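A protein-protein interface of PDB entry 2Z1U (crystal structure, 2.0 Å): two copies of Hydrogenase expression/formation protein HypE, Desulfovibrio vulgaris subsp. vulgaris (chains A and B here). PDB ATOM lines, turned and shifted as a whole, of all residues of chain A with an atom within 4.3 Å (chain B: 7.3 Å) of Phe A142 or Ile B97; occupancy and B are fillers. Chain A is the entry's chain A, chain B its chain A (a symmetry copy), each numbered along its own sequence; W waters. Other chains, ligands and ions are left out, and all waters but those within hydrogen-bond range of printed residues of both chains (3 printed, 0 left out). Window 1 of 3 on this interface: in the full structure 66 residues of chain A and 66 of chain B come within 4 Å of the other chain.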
ATOM      1  N   SER A  57      -2.866 -18.554  -7.603  1.00  0.00           N
ATOM      2  CA  SER A  57      -3.150 -19.135  -6.301  1.00  0.00           C
ATOM      3  C   SER A  57      -3.226 -20.642  -6.466  1.00  0.00           C
ATOM      4  O   SER A  57      -3.618 -21.127  -7.518  1.00  0.00           O
ATOM      5  CB  SER A  57      -4.463 -18.636  -5.707  1.00  0.00           C
ATOM      6  OG  SER A  57      -4.469 -17.237  -5.547  1.00  0.00           O
ATOM      7  N   TYR A  58      -2.882 -21.363  -5.400  1.00  0.00           N
ATOM      8  CA  TYR A  58      -2.788 -22.819  -5.414  1.00  0.00           C
ATOM      9  C   TYR A  58      -3.725 -23.368  -4.349  1.00  0.00           C
ATOM     10  O   TYR A  58      -3.704 -22.928  -3.200  1.00  0.00           O
ATOM     11  CB  TYR A  58      -1.324 -23.261  -5.235  1.00  0.00           C
ATOM     12  CG  TYR A  58      -0.484 -22.766  -6.400  1.00  0.00           C
ATOM     13  CD1 TYR A  58       0.073 -21.482  -6.374  1.00  0.00           C
ATOM     14  CD2 TYR A  58      -0.310 -23.549  -7.565  1.00  0.00           C
ATOM     15  CE1 TYR A  58       0.804 -20.991  -7.439  1.00  0.00           C
ATOM     16  CE2 TYR A  58       0.426 -23.053  -8.679  1.00  0.00           C
ATOM     17  CZ  TYR A  58       0.982 -21.765  -8.598  1.00  0.00           C
ATOM     18  OH  TYR A  58       1.743 -21.224  -9.628  1.00  0.00           O
ATOM     19  N   THR A  59      -4.586 -24.293  -4.764  1.00  0.00           N
ATOM     20  CA  THR A  59      -5.719 -24.741  -3.949  1.00  0.00           C
ATOM     21  C   THR A  59      -5.800 -26.273  -3.968  1.00  0.00           C
ATOM     22  O   THR A  59      -6.846 -26.848  -3.672  1.00  0.00           O
ATOM     23  CB  THR A  59      -7.071 -24.155  -4.471  1.00  0.00           C
ATOM     24  OG1 THR A  59      -7.226 -24.499  -5.846  1.00  0.00           O
ATOM     25  CG2 THR A  59      -7.117 -22.629  -4.344  1.00  0.00           C
ATOM     26  N   GLY A  95       2.035 -15.534  -0.680  1.00  0.00           N
ATOM     27  CA  GLY A  95       0.984 -15.111   0.216  1.00  0.00           C
ATOM     28  C   GLY A  95       0.315 -16.368   0.730  1.00  0.00           C
ATOM     29  O   GLY A  95      -0.328 -17.089  -0.033  1.00  0.00           O
ATOM     30  N   PHE A  96       0.520 -16.662   2.009  1.00  0.00           N
ATOM     31  CA  PHE A  96      -0.103 -17.819   2.660  1.00  0.00           C
ATOM     32  C   PHE A  96      -1.450 -17.428   3.238  1.00  0.00           C
ATOM     33  O   PHE A  96      -1.578 -16.369   3.860  1.00  0.00           O
ATOM     34  CB  PHE A  96       0.796 -18.380   3.782  1.00  0.00           C
ATOM     35  CG  PHE A  96       1.928 -19.241   3.287  1.00  0.00           C
ATOM     36  CD1 PHE A  96       3.085 -18.664   2.756  1.00  0.00           C
ATOM     37  CD2 PHE A  96       1.831 -20.625   3.327  1.00  0.00           C
ATOM     38  CE1 PHE A  96       4.137 -19.464   2.299  1.00  0.00           C
ATOM     39  CE2 PHE A  96       2.870 -21.431   2.867  1.00  0.00           C
ATOM     40  CZ  PHE A  96       4.024 -20.854   2.358  1.00  0.00           C
ATOM     41  N   ILE A  97      -2.451 -18.275   3.006  1.00  0.00           N
ATOM     42  CA  ILE A  97      -3.725 -18.201   3.728  1.00  0.00           C
ATOM     43  C   ILE A  97      -3.900 -19.517   4.488  1.00  0.00           C
ATOM     44  O   ILE A  97      -3.960 -20.585   3.885  1.00  0.00           O
ATOM     45  CB  ILE A  97      -4.925 -17.918   2.788  1.00  0.00           C
ATOM     46  CG1 ILE A  97      -4.691 -16.594   2.034  1.00  0.00           C
ATOM     47  CG2 ILE A  97      -6.248 -17.868   3.597  1.00  0.00           C
ATOM     48  CD1 ILE A  97      -5.637 -16.340   0.855  1.00  0.00           C
ATOM     49  N   CYS A 138     -11.260 -21.540   5.810  1.00  0.00           N
ATOM     50  CA  CYS A 138     -10.622 -22.109   4.618  1.00  0.00           C
ATOM     51  C   CYS A 138     -10.189 -23.547   4.878  1.00  0.00           C
ATOM     52  O   CYS A 138      -9.986 -23.941   6.032  1.00  0.00           O
ATOM     53  CB  CYS A 138      -9.435 -21.254   4.129  1.00  0.00           C
ATOM     54  SG  CYS A 138      -7.905 -21.451   5.056  1.00  0.00           S
ATOM     55  N   ASP A 139     -10.066 -24.331   3.809  1.00  0.00           N
ATOM     56  CA  ASP A 139      -9.651 -25.727   3.927  1.00  0.00           C
ATOM     57  C   ASP A 139      -8.131 -25.852   4.030  1.00  0.00           C
ATOM     58  O   ASP A 139      -7.439 -26.007   3.016  1.00  0.00           O
ATOM     59  CB  ASP A 139     -10.211 -26.563   2.763  1.00  0.00           C
ATOM     60  CG  ASP A 139      -9.874 -28.043   2.876  1.00  0.00           C
ATOM     61  OD1 ASP A 139      -9.641 -28.560   3.994  1.00  0.00           O
ATOM     62  OD2 ASP A 139      -9.846 -28.693   1.822  1.00  0.00           O
ATOM     63  N   MET A 141      -5.175 -24.673   3.807  1.00  0.00           N
ATOM     64  CA  MET A 141      -4.111 -23.835   3.254  1.00  0.00           C
ATOM     65  C   MET A 141      -4.240 -23.550   1.772  1.00  0.00           C
ATOM     66  O   MET A 141      -4.365 -24.481   0.957  1.00  0.00           O
ATOM     67  CB  MET A 141      -2.773 -24.531   3.503  1.00  0.00           C
ATOM     68  CG  MET A 141      -1.559 -23.891   2.881  1.00  0.00           C
ATOM     69  SD  MET A 141      -0.193 -25.004   3.224  1.00  0.00           S
ATOM     70  CE  MET A 141       1.067 -24.192   2.325  1.00  0.00           C
ATOM     71  N   PHE A 142      -4.166 -22.260   1.434  1.00  0.00           N
ATOM     72  CA  PHE A 142      -3.989 -21.819   0.060  1.00  0.00           C
ATOM     73  C   PHE A 142      -2.711 -20.999  -0.011  1.00  0.00           C
ATOM     74  O   PHE A 142      -2.304 -20.381   0.978  1.00  0.00           O
ATOM     75  CB  PHE A 142      -5.171 -20.959  -0.418  1.00  0.00           C
ATOM     76  CG  PHE A 142      -6.526 -21.610  -0.234  1.00  0.00           C
ATOM     77  CD1 PHE A 142      -7.584 -20.886   0.301  1.00  0.00           C
ATOM     78  CD2 PHE A 142      -6.736 -22.943  -0.578  1.00  0.00           C
ATOM     79  CE1 PHE A 142      -8.826 -21.472   0.480  1.00  0.00           C
ATOM     80  CE2 PHE A 142      -7.979 -23.542  -0.403  1.00  0.00           C
ATOM     81  CZ  PHE A 142      -9.021 -22.804   0.125  1.00  0.00           C
ATOM     82  N   ILE A 143      -2.078 -20.982  -1.181  1.00  0.00           N
ATOM     83  CA  ILE A 143      -0.881 -20.169  -1.369  1.00  0.00           C
ATOM     84  C   ILE A 143      -1.038 -19.417  -2.675  1.00  0.00           C
ATOM     85  O   ILE A 143      -1.402 -20.013  -3.702  1.00  0.00           O
ATOM     86  CB  ILE A 143       0.415 -21.039  -1.451  1.00  0.00           C
ATOM     87  CG1 ILE A 143       0.492 -22.051  -0.306  1.00  0.00           C
ATOM     88  CG2 ILE A 143       1.676 -20.154  -1.486  1.00  0.00           C
ATOM     89  CD1 ILE A 143       1.696 -23.043  -0.416  1.00  0.00           C
ATOM     90  N   ARG A 341     -10.077 -28.245  -7.664  1.00  0.00           N
ATOM     91  CA  ARG A 341      -8.887 -28.216  -6.829  1.00  0.00           C
ATOM     92  C   ARG A 341      -7.808 -29.225  -7.263  1.00  0.00           C
ATOM     93  O   ARG A 341      -7.151 -29.855  -6.428  1.00  0.00           O
ATOM     94  CB  ARG A 341      -9.304 -28.391  -5.364  1.00  0.00           C
ATOM     95  CG  ARG A 341     -10.084 -27.189  -4.843  1.00  0.00           C
ATOM     96  CD  ARG A 341     -10.466 -27.364  -3.396  1.00  0.00           C
ATOM     97  NE  ARG A 341      -9.308 -27.281  -2.516  1.00  0.00           N
ATOM     98  CZ  ARG A 341      -9.328 -27.581  -1.223  1.00  0.00           C
ATOM     99  NH1 ARG A 341     -10.455 -28.004  -0.644  1.00  0.00           N
ATOM    100  NH2 ARG A 341      -8.217 -27.468  -0.513  1.00  0.00           N
ATOM    101  N   LEU B   8     -22.231 -18.245  -8.867  1.00  0.00           N
ATOM    102  CA  LEU B   8     -20.847 -18.602  -9.214  1.00  0.00           C
ATOM    103  C   LEU B   8     -20.645 -20.124  -9.186  1.00  0.00           C
ATOM    104  O   LEU B   8     -20.352 -20.718  -8.141  1.00  0.00           O
ATOM    105  CB  LEU B   8     -19.805 -17.873  -8.350  1.00  0.00           C
ATOM    106  CG  LEU B   8     -18.351 -18.108  -8.788  1.00  0.00           C
ATOM    107  CD1 LEU B   8     -17.880 -17.155  -9.895  1.00  0.00           C
ATOM    108  CD2 LEU B   8     -17.426 -18.027  -7.600  1.00  0.00           C
ATOM    109  N   SER B  57      -2.513 -10.888   1.078  1.00  0.00           N
ATOM    110  CA  SER B  57      -3.826 -11.480   0.877  1.00  0.00           C
ATOM    111  C   SER B  57      -4.811 -10.753   1.773  1.00  0.00           C
ATOM    112  O   SER B  57      -4.442 -10.285   2.842  1.00  0.00           O
ATOM    113  CB  SER B  57      -3.859 -12.967   1.210  1.00  0.00           C
ATOM    114  OG  SER B  57      -2.948 -13.701   0.426  1.00  0.00           O
ATOM    115  N   GLY B  95      -5.084 -12.196  -7.451  1.00  0.00           N
ATOM    116  CA  GLY B  95      -5.382 -13.610  -7.418  1.00  0.00           C
ATOM    117  C   GLY B  95      -6.645 -13.772  -6.600  1.00  0.00           C
ATOM    118  O   GLY B  95      -6.643 -13.523  -5.395  1.00  0.00           O
ATOM    119  N   PHE B  96      -7.736 -14.129  -7.268  1.00  0.00           N
ATOM    120  CA  PHE B  96      -9.020 -14.373  -6.604  1.00  0.00           C
ATOM    121  C   PHE B  96      -9.120 -15.828  -6.185  1.00  0.00           C
ATOM    122  O   PHE B  96      -8.774 -16.726  -6.957  1.00  0.00           O
ATOM    123  CB  PHE B  96     -10.204 -14.022  -7.530  1.00  0.00           C
ATOM    124  CG  PHE B  96     -10.502 -12.547  -7.610  1.00  0.00           C
ATOM    125  CD1 PHE B  96      -9.726 -11.705  -8.412  1.00  0.00           C
ATOM    126  CD2 PHE B  96     -11.537 -11.995  -6.870  1.00  0.00           C
ATOM    127  CE1 PHE B  96     -10.003 -10.337  -8.487  1.00  0.00           C
ATOM    128  CE2 PHE B  96     -11.818 -10.632  -6.932  1.00  0.00           C
ATOM    129  CZ  PHE B  96     -11.057  -9.803  -7.743  1.00  0.00           C
ATOM    130  N   ILE B  97      -9.572 -16.047  -4.951  1.00  0.00           N
ATOM    131  CA  ILE B  97     -10.003 -17.374  -4.498  1.00  0.00           C
ATOM    132  C   ILE B  97     -11.481 -17.273  -4.119  1.00  0.00           C
ATOM    133  O   ILE B  97     -11.847 -16.518  -3.221  1.00  0.00           O
ATOM    134  CB  ILE B  97      -9.144 -17.908  -3.323  1.00  0.00           C
ATOM    135  CG1 ILE B  97      -7.665 -17.974  -3.750  1.00  0.00           C
ATOM    136  CG2 ILE B  97      -9.652 -19.302  -2.870  1.00  0.00           C
ATOM    137  CD1 ILE B  97      -6.666 -18.189  -2.607  1.00  0.00           C
ATOM    138  N   LEU B  98     -12.328 -18.017  -4.824  1.00  0.00           N
ATOM    139  CA  LEU B  98     -13.770 -17.823  -4.708  1.00  0.00           C
ATOM    140  C   LEU B  98     -14.499 -19.097  -4.334  1.00  0.00           C
ATOM    141  O   LEU B  98     -14.121 -20.194  -4.765  1.00  0.00           O
ATOM    142  CB  LEU B  98     -14.330 -17.272  -6.020  1.00  0.00           C
ATOM    143  CG  LEU B  98     -13.776 -15.925  -6.508  1.00  0.00           C
ATOM    144  CD1 LEU B  98     -14.082 -15.710  -7.998  1.00  0.00           C
ATOM    145  CD2 LEU B  98     -14.327 -14.787  -5.665  1.00  0.00           C
ATOM    146  N   GLU B  99     -15.542 -18.938  -3.525  1.00  0.00           N
ATOM    147  CA  GLU B  99     -16.389 -20.052  -3.116  1.00  0.00           C
ATOM    148  C   GLU B  99     -17.501 -20.290  -4.142  1.00  0.00           C
ATOM    149  O   GLU B  99     -18.228 -19.356  -4.513  1.00  0.00           O
ATOM    150  CB  GLU B  99     -16.991 -19.780  -1.731  1.00  0.00           C
ATOM    151  CG  GLU B  99     -17.810 -20.947  -1.191  1.00  0.00           C
ATOM    152  CD  GLU B  99     -18.376 -20.714   0.188  1.00  0.00           C
ATOM    153  OE1 GLU B  99     -18.623 -21.725   0.887  1.00  0.00           O
ATOM    154  OE2 GLU B  99     -18.591 -19.545   0.575  1.00  0.00           O
ATOM    155  N   LEU B 102     -21.219 -18.482  -4.625  1.00  0.00           N
ATOM    156  CA  LEU B 102     -21.135 -17.049  -4.350  1.00  0.00           C
ATOM    157  C   LEU B 102     -22.048 -16.233  -5.269  1.00  0.00           C
ATOM    158  O   LEU B 102     -22.053 -16.429  -6.486  1.00  0.00           O
ATOM    159  CB  LEU B 102     -19.681 -16.573  -4.487  1.00  0.00           C
ATOM    160  CG  LEU B 102     -19.087 -15.379  -3.716  1.00  0.00           C
ATOM    161  CD1 LEU B 102     -18.559 -14.290  -4.656  1.00  0.00           C
ATOM    162  CD2 LEU B 102     -19.994 -14.794  -2.646  1.00  0.00           C
ATOM    163  N   ASP B 129      -5.415 -14.165 -11.584  1.00  0.00           N
ATOM    164  CA  ASP B 129      -5.774 -15.568 -11.468  1.00  0.00           C
ATOM    165  C   ASP B 129      -7.120 -15.651 -10.786  1.00  0.00           C
ATOM    166  O   ASP B 129      -7.450 -14.800  -9.976  1.00  0.00           O
ATOM    167  CB  ASP B 129      -4.728 -16.326 -10.639  1.00  0.00           C
ATOM    168  CG  ASP B 129      -4.975 -17.828 -10.629  1.00  0.00           C
ATOM    169  OD1 ASP B 129      -5.070 -18.420 -11.737  1.00  0.00           O
ATOM    170  OD2 ASP B 129      -5.059 -18.417  -9.533  1.00  0.00           O
ATOM    171  N   THR B 130      -7.869 -16.701 -11.099  1.00  0.00           N
ATOM    172  CA  THR B 130      -9.199 -16.908 -10.569  1.00  0.00           C
ATOM    173  C   THR B 130      -9.343 -18.400 -10.274  1.00  0.00           C
ATOM    174  O   THR B 130      -9.364 -19.243 -11.188  1.00  0.00           O
ATOM    175  CB  THR B 130     -10.294 -16.474 -11.589  1.00  0.00           C
ATOM    176  OG1 THR B 130      -9.990 -15.156 -12.080  1.00  0.00           O
ATOM    177  CG2 THR B 130     -11.690 -16.479 -10.922  1.00  0.00           C
ATOM    178  N   LYS B 131      -9.432 -18.715  -8.987  1.00  0.00           N
ATOM    179  CA  LYS B 131      -9.652 -20.076  -8.534  1.00  0.00           C
ATOM    180  C   LYS B 131     -11.030 -20.086  -7.866  1.00  0.00           C
ATOM    181  O   LYS B 131     -11.344 -19.208  -7.067  1.00  0.00           O
ATOM    182  CB  LYS B 131      -8.546 -20.523  -7.546  1.00  0.00           C
ATOM    183  CG  LYS B 131      -7.109 -20.742  -8.121  1.00  0.00           C
ATOM    184  CD  LYS B 131      -7.095 -21.737  -9.312  1.00  0.00           C
ATOM    185  CE  LYS B 131      -5.717 -22.223  -9.745  1.00  0.00           C
ATOM    186  NZ  LYS B 131      -4.733 -21.168 -10.197  1.00  0.00           N
ATOM    187  N   VAL B 132     -11.854 -21.063  -8.230  1.00  0.00           N
ATOM    188  CA  VAL B 132     -13.145 -21.276  -7.581  1.00  0.00           C
ATOM    189  C   VAL B 132     -13.093 -22.623  -6.868  1.00  0.00           C
ATOM    190  O   VAL B 132     -12.867 -23.654  -7.498  1.00  0.00           O
ATOM    191  CB  VAL B 132     -14.328 -21.253  -8.592  1.00  0.00           C
ATOM    192  CG1 VAL B 132     -15.672 -21.393  -7.859  1.00  0.00           C
ATOM    193  CG2 VAL B 132     -14.316 -19.962  -9.423  1.00  0.00           C
ATOM    194  N   VAL B 133     -13.290 -22.614  -5.555  1.00  0.00           N
ATOM    195  CA  VAL B 133     -13.254 -23.854  -4.762  1.00  0.00           C
ATOM    196  C   VAL B 133     -14.681 -24.312  -4.376  1.00  0.00           C
ATOM    197  O   VAL B 133     -15.590 -23.481  -4.314  1.00  0.00           O
ATOM    198  CB  VAL B 133     -12.338 -23.690  -3.502  1.00  0.00           C
ATOM    199  CG1 VAL B 133     -10.891 -23.516  -3.920  1.00  0.00           C
ATOM    200  CG2 VAL B 133     -12.806 -22.508  -2.644  1.00  0.00           C
ATOM    201  N   GLY B 136     -17.893 -24.401   0.942  1.00  0.00           N
ATOM    202  CA  GLY B 136     -17.303 -24.694   2.246  1.00  0.00           C
ATOM    203  C   GLY B 136     -15.782 -24.692   2.300  1.00  0.00           C
ATOM    204  O   GLY B 136     -15.203 -24.602   3.391  1.00  0.00           O
ATOM    205  N   ALA B 137     -15.129 -24.770   1.138  1.00  0.00           N
ATOM    206  CA  ALA B 137     -13.666 -24.799   1.081  1.00  0.00           C
ATOM    207  C   ALA B 137     -13.034 -23.442   1.403  1.00  0.00           C
ATOM    208  O   ALA B 137     -11.859 -23.372   1.791  1.00  0.00           O
ATOM    209  CB  ALA B 137     -13.188 -25.325  -0.257  1.00  0.00           C
ATOM    210  N   CYS B 138     -13.806 -22.365   1.236  1.00  0.00           N
ATOM    211  CA  CYS B 138     -13.411 -21.037   1.716  1.00  0.00           C
ATOM    212  C   CYS B 138     -14.640 -20.183   2.005  1.00  0.00           C
ATOM    213  O   CYS B 138     -15.719 -20.433   1.454  1.00  0.00           O
ATOM    214  CB  CYS B 138     -12.461 -20.322   0.732  1.00  0.00           C
ATOM    215  SG  CYS B 138     -13.251 -19.580  -0.706  1.00  0.00           S
ATOM    216  N   ASP B 139     -14.481 -19.193   2.879  1.00  0.00           N
ATOM    217  CA  ASP B 139     -15.583 -18.301   3.235  1.00  0.00           C
ATOM    218  C   ASP B 139     -15.756 -17.187   2.203  1.00  0.00           C
ATOM    219  O   ASP B 139     -15.181 -16.100   2.343  1.00  0.00           O
ATOM    220  CB  ASP B 139     -15.393 -17.736   4.653  1.00  0.00           C
ATOM    221  CG  ASP B 139     -16.551 -16.860   5.107  1.00  0.00           C
ATOM    222  OD1 ASP B 139     -17.695 -17.012   4.617  1.00  0.00           O
ATOM    223  OD2 ASP B 139     -16.304 -16.009   5.971  1.00  0.00           O
ATOM    224  N   LYS B 140     -16.528 -17.490   1.152  1.00  0.00           N
ATOM    225  CA  LYS B 140     -16.932 -16.528   0.099  1.00  0.00           C
ATOM    226  C   LYS B 140     -15.808 -16.096  -0.842  1.00  0.00           C
ATOM    227  O   LYS B 140     -15.889 -16.314  -2.055  1.00  0.00           O
ATOM    228  CB  LYS B 140     -17.610 -15.272   0.675  1.00  0.00           C
ATOM    229  CG  LYS B 140     -18.751 -15.499   1.650  1.00  0.00           C
ATOM    230  CD  LYS B 140     -19.429 -14.177   1.980  1.00  0.00           C
ATOM    231  CE  LYS B 140     -19.790 -14.079   3.450  1.00  0.00           C
ATOM    232  NZ  LYS B 140     -20.346 -15.331   3.990  1.00  0.00           N
ATOM    233  N   MET B 141     -14.766 -15.466  -0.294  1.00  0.00           N
ATOM    234  CA  MET B 141     -13.784 -14.801  -1.152  1.00  0.00           C
ATOM    235  C   MET B 141     -12.561 -14.283  -0.423  1.00  0.00           C
ATOM    236  O   MET B 141     -12.682 -13.533   0.560  1.00  0.00           O
ATOM    237  CB  MET B 141     -14.472 -13.628  -1.849  1.00  0.00           C
ATOM    238  CG  MET B 141     -13.589 -12.727  -2.672  1.00  0.00           C
ATOM    239  SD  MET B 141     -14.645 -11.387  -3.229  1.00  0.00           S
ATOM    240  CE  MET B 141     -13.447 -10.393  -4.025  1.00  0.00           C
ATOM    241  N   PHE B 142     -11.390 -14.658  -0.944  1.00  0.00           N
ATOM    242  CA  PHE B 142     -10.129 -14.043  -0.561  1.00  0.00           C
ATOM    243  C   PHE B 142      -9.493 -13.456  -1.810  1.00  0.00           C
ATOM    244  O   PHE B 142      -9.721 -13.944  -2.922  1.00  0.00           O
ATOM    245  CB  PHE B 142      -9.167 -15.065   0.069  1.00  0.00           C
ATOM    246  CG  PHE B 142      -9.757 -15.842   1.225  1.00  0.00           C
ATOM    247  CD1 PHE B 142      -9.588 -17.219   1.303  1.00  0.00           C
ATOM    248  CD2 PHE B 142     -10.492 -15.203   2.221  1.00  0.00           C
ATOM    249  CE1 PHE B 142     -10.128 -17.943   2.353  1.00  0.00           C
ATOM    250  CE2 PHE B 142     -11.039 -15.919   3.279  1.00  0.00           C
ATOM    251  CZ  PHE B 142     -10.855 -17.288   3.343  1.00  0.00           C
ATOM    252  N   ILE B 143      -8.685 -12.414  -1.634  1.00  0.00           N
ATOM    253  CA  ILE B 143      -7.971 -11.825  -2.762  1.00  0.00           C
ATOM    254  C   ILE B 143      -6.528 -11.632  -2.342  1.00  0.00           C
ATOM    255  O   ILE B 143      -6.257 -11.104  -1.251  1.00  0.00           O
ATOM    256  CB  ILE B 143      -8.559 -10.434  -3.168  1.00  0.00           C
ATOM    257  CG1 ILE B 143     -10.081 -10.484  -3.317  1.00  0.00           C
ATOM    258  CG2 ILE B 143      -7.899  -9.907  -4.457  1.00  0.00           C
ATOM    259  CD1 ILE B 143     -10.738  -9.090  -3.584  1.00  0.00           C
ATOM    260  N   ASN B 144      -5.604 -12.067  -3.195  1.00  0.00           N
ATOM    261  CA  ASN B 144      -4.230 -11.645  -3.064  1.00  0.00           C
ATOM    262  C   ASN B 144      -3.920 -10.586  -4.115  1.00  0.00           C
ATOM    263  O   ASN B 144      -4.348 -10.693  -5.283  1.00  0.00           O
ATOM    264  CB  ASN B 144      -3.273 -12.829  -3.229  1.00  0.00           C
ATOM    265  CG  ASN B 144      -1.811 -12.400  -3.134  1.00  0.00           C
ATOM    266  OD1 ASN B 144      -1.261 -11.888  -4.100  1.00  0.00           O
ATOM    267  ND2 ASN B 144      -1.187 -12.609  -1.969  1.00  0.00           N
HETATM  268  O   HOH W   1      -2.483 -22.691 -10.274  1.00  0.00           O
HETATM  269  O   HOH W   2      -6.118 -16.766  -7.601  1.00  0.00           O
HETATM  270  O   HOH W   3      -1.188 -14.091   2.403  1.00  0.00           O
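Hydrophobic or aromatic side chains of chain A that line the printed part of chain B: Ile A97 and Phe A142. Among the printed residues, 15 pairs touch across the chains. Among the printed residues, no Asp or Glu carboxylate lies within 4 Å of a Lys or Arg side-chain nitrogen of the other chain.
Ser A57 touches Ile B97, and with the chains exchanged Ile A97 touches Ser B57. Ile A97 touches Phe B142, and with the chains exchanged Phe A142 touches Ile B97. Cys A138 touches Phe B142, and with the chains exchanged Phe A142 touches Cys B138. Positions printed for both chains: 57, 95, 96, 97, 138, 139, 141, 142 and 143.
OG of Ser A57 touches CG1 of Ile B97, at 3.7 Å. Val B133 touches Thr A59. Ile A97 touches Ser B57 (CG1 to OG, 3.7 Å). Ile A97 touches Phe B142. Cys A138 touches Phe B142. CB of Phe A142 touches CD1 of Ile B97 (3.8 Å). Ala B137 touches Phe A142 (O to CZ, 3.3 Å). CE1 of Phe A142 touches CB of Cys B138, 3.8 Å away. Val B133 touches Arg A341. Arg A341 touches Ala B137.
Printed residues of chain B within 4 Å of Ser A57: Ile B97 (3.7 Å), Asp B129 (2.9 Å) and Lys B131 (2.9 Å). Tyr A58 touches none of the printed residues of chain B. Of the printed residues of chain B, Ile A97 touches Ser B57 (3.7 Å) and Phe B142 (3.8 Å). Ile B97 touches just these residues of chain A: Ser A57 and Phe A142. Of the printed residues of chain A, Lys B131 touches Ser A57 (2.9 Å). Of the printed residues of chain A, Cys B138 touches Phe A142 (3.8 Å).
N of Asp A139 is in hydrogen-bond range of O of Ala B137 (2.9 Å). NZ of Lys B131 lies within hydrogen-bond range of O of Ser A57 (2.9 Å). The side-chain carboxylate (OD2) of Asp B129 is in hydrogen-bond range of the backbone NH (N) of Ser A57 (2.9 Å).
The guanidinium group (NH1) of Arg A341 is in salt-bridge range of the side-chain carboxylate (OD2) of Asp A139 (2.6 Å). The side-chain carboxylate (OD2) of Asp B129 lies within salt-bridge range of the side-chain amino group (NZ) of Lys B131. ND2 of Asn B144 lies within hydrogen-bond range of OG of Ser B57 (3.2 Å). The backbone carbonyl oxygen (O) of Phe B96 is in hydrogen-bond range of the backbone NH (N) of Lys B131 (2.9 Å). The backbone carbonyl oxygen of Thr A59 is in hydrogen-bond range of the guanidinium group of Arg A341 (2.8 Å). The backbone NH of Ile A97 is in hydrogen-bond range of the backbone carbonyl oxygen of Phe A142, 2.9 Å away.
Water W3 lies within hydrogen-bond range of OG of Ser B57 (2.7 Å) and O of Phe A96 (2.7 Å). Water W2 lies within hydrogen-bond range of the side-chain hydroxyl of Ser A57 (2.7 Å), the backbone carbonyl oxygen of Phe B96 (2.7 Å) and the side-chain carboxylate of Asp B129 (2.8 Å). Water W1 lies within hydrogen-bond range of the side-chain amino group (NZ) of Lys B131 (2.7 Å) and the backbone carbonyl oxygen (O) of Ser A57 (3.4 Å).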
